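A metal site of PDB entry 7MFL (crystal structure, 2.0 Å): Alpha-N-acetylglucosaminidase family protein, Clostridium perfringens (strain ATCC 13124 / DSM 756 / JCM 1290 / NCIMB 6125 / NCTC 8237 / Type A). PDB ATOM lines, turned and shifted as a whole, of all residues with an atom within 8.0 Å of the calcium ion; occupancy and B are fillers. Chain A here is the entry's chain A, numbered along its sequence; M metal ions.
The calcium ion is bound by O of Asp 36 (2.3 Å), O of Leu 31 (2.3 Å), OE2 of Glu 132 (2.4 Å), O of Thr 39 (2.4 Å), O of Ala 131 (2.5 Å), OD1 of Asp 34 (2.5 Å) and OG1 of Thr 39 (2.6 Å). The calcium ion has seven donor atoms within binding distance.
The nearest printed residue that does not touch the calcium ion is Tyr 40 (4.2 Å).
The backbone NH (N) of Ala 131 is in hydrogen-bond range of the backbone carbonyl oxygen (O) of Phe 66, at 2.8 Å. The side-chain carboxylate (OD1) of Asp 36 is in hydrogen-bond range of the side-chain hydroxyl (OG) of Ser 38 (2.6 Å). The backbone NH (N) of Phe 66 sits at hydrogen-bond distance from the backbone carbonyl oxygen (O) of Glu 132 (2.8 Å). The side-chain carboxylate of Glu 132 is in hydrogen-bond range of the backbone NH of Gly 35 (2.9 Å).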
ATOM      1  N   THR A  28     -17.154 -13.121 -20.812  1.00  0.00           N
ATOM      2  CA  THR A  28     -16.020 -13.562 -20.025  1.00  0.00           C
ATOM      3  C   THR A  28     -16.442 -13.884 -18.592  1.00  0.00           C
ATOM      4  O   THR A  28     -17.541 -13.563 -18.153  1.00  0.00           O
ATOM      5  CB  THR A  28     -14.925 -12.485 -20.028  1.00  0.00           C
ATOM      6  OG1 THR A  28     -15.479 -11.242 -19.602  1.00  0.00           O
ATOM      7  CG2 THR A  28     -14.350 -12.325 -21.431  1.00  0.00           C
ATOM      8  N   ALA A  29     -15.528 -14.534 -17.870  1.00  0.00           N
ATOM      9  CA  ALA A  29     -15.835 -15.034 -16.532  1.00  0.00           C
ATOM     10  C   ALA A  29     -16.224 -13.913 -15.584  1.00  0.00           C
ATOM     11  O   ALA A  29     -17.145 -14.065 -14.772  1.00  0.00           O
ATOM     12  CB  ALA A  29     -14.648 -15.811 -15.980  1.00  0.00           C
ATOM     13  N   ASP A  30     -15.534 -12.764 -15.671  1.00  0.00           N
ATOM     14  CA  ASP A  30     -15.797 -11.656 -14.772  1.00  0.00           C
ATOM     15  C   ASP A  30     -17.237 -11.173 -14.849  1.00  0.00           C
ATOM     16  O   ASP A  30     -17.732 -10.558 -13.887  1.00  0.00           O
ATOM     17  CB  ASP A  30     -14.853 -10.499 -15.077  1.00  0.00           C
ATOM     18  CG  ASP A  30     -14.824 -10.148 -16.548  1.00  0.00           C
ATOM     19  OD1 ASP A  30     -15.488  -9.162 -16.934  1.00  0.00           O
ATOM     20  OD2 ASP A  30     -14.130 -10.851 -17.319  1.00  0.00           O
ATOM     21  N   LEU A  31     -17.927 -11.426 -15.961  1.00  0.00           N
ATOM     22  CA  LEU A  31     -19.326 -11.033 -16.090  1.00  0.00           C
ATOM     23  C   LEU A  31     -20.254 -11.849 -15.212  1.00  0.00           C
ATOM     24  O   LEU A  31     -21.441 -11.503 -15.110  1.00  0.00           O
ATOM     25  CB  LEU A  31     -19.763 -11.140 -17.555  1.00  0.00           C
ATOM     26  CG  LEU A  31     -19.002 -10.205 -18.502  1.00  0.00           C
ATOM     27  CD1 LEU A  31     -19.519 -10.350 -19.920  1.00  0.00           C
ATOM     28  CD2 LEU A  31     -19.106  -8.761 -18.034  1.00  0.00           C
ATOM     29  N   ALA A  32     -19.761 -12.920 -14.586  1.00  0.00           N
ATOM     30  CA  ALA A  32     -20.576 -13.668 -13.631  1.00  0.00           C
ATOM     31  C   ALA A  32     -20.647 -12.998 -12.268  1.00  0.00           C
ATOM     32  O   ALA A  32     -21.479 -13.396 -11.449  1.00  0.00           O
ATOM     33  CB  ALA A  32     -20.026 -15.087 -13.477  1.00  0.00           C
ATOM     34  N   ILE A  33     -19.798 -12.003 -11.998  1.00  0.00           N
ATOM     35  CA  ILE A  33     -19.728 -11.392 -10.673  1.00  0.00           C
ATOM     36  C   ILE A  33     -19.682  -9.877 -10.766  1.00  0.00           C
ATOM     37  O   ILE A  33     -19.151  -9.215  -9.862  1.00  0.00           O
ATOM     38  CB  ILE A  33     -18.501 -11.925  -9.898  1.00  0.00           C
ATOM     39  CG1 ILE A  33     -17.213 -11.628 -10.672  1.00  0.00           C
ATOM     40  CG2 ILE A  33     -18.630 -13.414  -9.618  1.00  0.00           C
ATOM     41  CD1 ILE A  33     -15.976 -11.646  -9.810  1.00  0.00           C
ATOM     42  N   ASP A  34     -20.215  -9.312 -11.837  1.00  0.00           N
ATOM     43  CA  ASP A  34     -20.180  -7.868 -12.018  1.00  0.00           C
ATOM     44  C   ASP A  34     -21.431  -7.168 -11.504  1.00  0.00           C
ATOM     45  O   ASP A  34     -21.617  -5.975 -11.770  1.00  0.00           O
ATOM     46  CB  ASP A  34     -19.942  -7.510 -13.497  1.00  0.00           C
ATOM     47  CG  ASP A  34     -21.118  -7.875 -14.395  1.00  0.00           C
ATOM     48  OD1 ASP A  34     -22.063  -8.543 -13.927  1.00  0.00           O
ATOM     49  OD2 ASP A  34     -21.096  -7.482 -15.579  1.00  0.00           O
ATOM     50  N   GLY A  35     -22.283  -7.874 -10.761  1.00  0.00           N
ATOM     51  CA  GLY A  35     -23.478  -7.283 -10.192  1.00  0.00           C
ATOM     52  C   GLY A  35     -24.561  -6.932 -11.187  1.00  0.00           C
ATOM     53  O   GLY A  35     -25.516  -6.228 -10.823  1.00  0.00           O
ATOM     54  N   ASP A  36     -24.464  -7.403 -12.430  1.00  0.00           N
ATOM     55  CA  ASP A  36     -25.378  -7.034 -13.508  1.00  0.00           C
ATOM     56  C   ASP A  36     -26.031  -8.310 -14.041  1.00  0.00           C
ATOM     57  O   ASP A  36     -25.352  -9.167 -14.620  1.00  0.00           O
ATOM     58  CB  ASP A  36     -24.625  -6.294 -14.614  1.00  0.00           C
ATOM     59  CG  ASP A  36     -25.543  -5.679 -15.649  1.00  0.00           C
ATOM     60  OD1 ASP A  36     -26.752  -5.979 -15.636  1.00  0.00           O
ATOM     61  OD2 ASP A  36     -25.052  -4.880 -16.473  1.00  0.00           O
ATOM     62  N   LEU A  37     -27.347  -8.418 -13.869  1.00  0.00           N
ATOM     63  CA  LEU A  37     -28.064  -9.604 -14.324  1.00  0.00           C
ATOM     64  C   LEU A  37     -28.170  -9.688 -15.843  1.00  0.00           C
ATOM     65  O   LEU A  37     -28.574 -10.733 -16.358  1.00  0.00           O
ATOM     66  CB  LEU A  37     -29.454  -9.639 -13.700  1.00  0.00           C
ATOM     67  CG  LEU A  37     -29.473  -9.936 -12.209  1.00  0.00           C
ATOM     68  CD1 LEU A  37     -30.887  -9.875 -11.665  1.00  0.00           C
ATOM     69  CD2 LEU A  37     -28.854 -11.299 -11.924  1.00  0.00           C
ATOM     70  N   SER A  38     -27.823  -8.620 -16.566  1.00  0.00           N
ATOM     71  CA  SER A  38     -27.907  -8.614 -18.020  1.00  0.00           C
ATOM     72  C   SER A  38     -26.621  -9.062 -18.696  1.00  0.00           C
ATOM     73  O   SER A  38     -26.608  -9.202 -19.924  1.00  0.00           O
ATOM     74  CB  SER A  38     -28.297  -7.207 -18.517  1.00  0.00           C
ATOM     75  OG  SER A  38     -27.296  -6.269 -18.186  1.00  0.00           O
ATOM     76  N   THR A  39     -25.547  -9.269 -17.941  1.00  0.00           N
ATOM     77  CA  THR A  39     -24.293  -9.789 -18.458  1.00  0.00           C
ATOM     78  C   THR A  39     -24.034 -11.153 -17.844  1.00  0.00           C
ATOM     79  O   THR A  39     -24.425 -11.421 -16.704  1.00  0.00           O
ATOM     80  CB  THR A  39     -23.125  -8.849 -18.150  1.00  0.00           C
ATOM     81  OG1 THR A  39     -22.897  -8.810 -16.737  1.00  0.00           O
ATOM     82  CG2 THR A  39     -23.437  -7.437 -18.640  1.00  0.00           C
ATOM     83  N   TYR A  40     -23.364 -12.021 -18.598  1.00  0.00           N
ATOM     84  CA  TYR A  40     -23.187 -13.389 -18.150  1.00  0.00           C
ATOM     85  C   TYR A  40     -21.892 -13.973 -18.704  1.00  0.00           C
ATOM     86  O   TYR A  40     -21.462 -13.628 -19.805  1.00  0.00           O
ATOM     87  CB  TYR A  40     -24.373 -14.273 -18.569  1.00  0.00           C
ATOM     88  CG  TYR A  40     -24.667 -14.265 -20.052  1.00  0.00           C
ATOM     89  CD1 TYR A  40     -25.548 -13.342 -20.595  1.00  0.00           C
ATOM     90  CD2 TYR A  40     -24.062 -15.174 -20.902  1.00  0.00           C
ATOM     91  CE1 TYR A  40     -25.821 -13.322 -21.949  1.00  0.00           C
ATOM     92  CE2 TYR A  40     -24.327 -15.169 -22.270  1.00  0.00           C
ATOM     93  CZ  TYR A  40     -25.210 -14.236 -22.786  1.00  0.00           C
ATOM     94  OH  TYR A  40     -25.478 -14.220 -24.127  1.00  0.00           O
ATOM     95  N   TRP A  41     -21.278 -14.850 -17.912  1.00  0.00           N
ATOM     96  CA  TRP A  41     -20.281 -15.769 -18.446  1.00  0.00           C
ATOM     97  C   TRP A  41     -20.995 -16.889 -19.186  1.00  0.00           C
ATOM     98  O   TRP A  41     -22.066 -17.346 -18.760  1.00  0.00           O
ATOM     99  CB  TRP A  41     -19.420 -16.360 -17.332  1.00  0.00           C
ATOM    100  CG  TRP A  41     -18.665 -17.591 -17.761  1.00  0.00           C
ATOM    101  CD1 TRP A  41     -17.500 -17.631 -18.479  1.00  0.00           C
ATOM    102  CD2 TRP A  41     -19.042 -18.963 -17.523  1.00  0.00           C
ATOM    103  NE1 TRP A  41     -17.119 -18.933 -18.696  1.00  0.00           N
ATOM    104  CE2 TRP A  41     -18.043 -19.771 -18.113  1.00  0.00           C
ATOM    105  CE3 TRP A  41     -20.105 -19.580 -16.862  1.00  0.00           C
ATOM    106  CZ2 TRP A  41     -18.087 -21.166 -18.065  1.00  0.00           C
ATOM    107  CZ3 TRP A  41     -20.140 -20.964 -16.814  1.00  0.00           C
ATOM    108  CH2 TRP A  41     -19.137 -21.739 -17.412  1.00  0.00           C
ATOM    109  N   PHE A  66     -27.867 -16.858 -10.492  1.00  0.00           N
ATOM    110  CA  PHE A  66     -28.788 -16.450 -11.539  1.00  0.00           C
ATOM    111  C   PHE A  66     -28.257 -16.919 -12.888  1.00  0.00           C
ATOM    112  O   PHE A  66     -27.040 -16.888 -13.128  1.00  0.00           O
ATOM    113  CB  PHE A  66     -28.956 -14.930 -11.579  1.00  0.00           C
ATOM    114  CG  PHE A  66     -29.515 -14.328 -10.313  1.00  0.00           C
ATOM    115  CD1 PHE A  66     -30.854 -14.011 -10.220  1.00  0.00           C
ATOM    116  CD2 PHE A  66     -28.693 -14.074  -9.234  1.00  0.00           C
ATOM    117  CE1 PHE A  66     -31.377 -13.454  -9.064  1.00  0.00           C
ATOM    118  CE2 PHE A  66     -29.201 -13.518  -8.076  1.00  0.00           C
ATOM    119  CZ  PHE A  66     -30.540 -13.211  -7.993  1.00  0.00           C
ATOM    120  N   ILE A 130     -23.703 -18.364 -16.402  1.00  0.00           N
ATOM    121  CA  ILE A 130     -24.025 -17.828 -15.083  1.00  0.00           C
ATOM    122  C   ILE A 130     -24.130 -16.318 -15.232  1.00  0.00           C
ATOM    123  O   ILE A 130     -23.150 -15.657 -15.574  1.00  0.00           O
ATOM    124  CB  ILE A 130     -22.974 -18.208 -14.019  1.00  0.00           C
ATOM    125  CG1 ILE A 130     -22.980 -19.715 -13.765  1.00  0.00           C
ATOM    126  CG2 ILE A 130     -23.235 -17.445 -12.730  1.00  0.00           C
ATOM    127  CD1 ILE A 130     -21.835 -20.207 -12.927  1.00  0.00           C
ATOM    128  N   ALA A 131     -25.322 -15.776 -14.990  1.00  0.00           N
ATOM    129  CA  ALA A 131     -25.514 -14.334 -15.067  1.00  0.00           C
ATOM    130  C   ALA A 131     -24.901 -13.642 -13.854  1.00  0.00           C
ATOM    131  O   ALA A 131     -24.164 -12.666 -13.997  1.00  0.00           O
ATOM    132  CB  ALA A 131     -26.997 -13.995 -15.201  1.00  0.00           C
ATOM    133  N   GLU A 132     -25.199 -14.141 -12.655  1.00  0.00           N
ATOM    134  CA  GLU A 132     -24.646 -13.606 -11.424  1.00  0.00           C
ATOM    135  C   GLU A 132     -24.546 -14.723 -10.405  1.00  0.00           C
ATOM    136  O   GLU A 132     -25.372 -15.644 -10.375  1.00  0.00           O
ATOM    137  CB  GLU A 132     -25.497 -12.461 -10.853  1.00  0.00           C
ATOM    138  CG  GLU A 132     -25.234 -11.097 -11.475  1.00  0.00           C
ATOM    139  CD  GLU A 132     -23.787 -10.672 -11.345  1.00  0.00           C
ATOM    140  OE1 GLU A 132     -23.285 -10.570 -10.205  1.00  0.00           O
ATOM    141  OE2 GLU A 132     -23.138 -10.440 -12.391  1.00  0.00           O
ATOM    142  N   ILE A 133     -23.506 -14.652  -9.561  1.00  0.00           N
ATOM    143  CA  ILE A 133     -23.397 -15.504  -8.394  1.00  0.00           C
ATOM    144  C   ILE A 133     -23.053 -14.637  -7.189  1.00  0.00           C
ATOM    145  O   ILE A 133     -22.077 -13.884  -7.230  1.00  0.00           O
ATOM    146  CB  ILE A 133     -22.359 -16.632  -8.586  1.00  0.00           C
ATOM    147  CG1 ILE A 133     -22.159 -17.383  -7.261  1.00  0.00           C
ATOM    148  CG2 ILE A 133     -21.040 -16.086  -9.115  1.00  0.00           C
ATOM    149  CD1 ILE A 133     -21.259 -18.595  -7.378  1.00  0.00           C
HETATM  150 CA    CA M   1     -23.454 -10.431 -14.750  1.00  0.00          CA
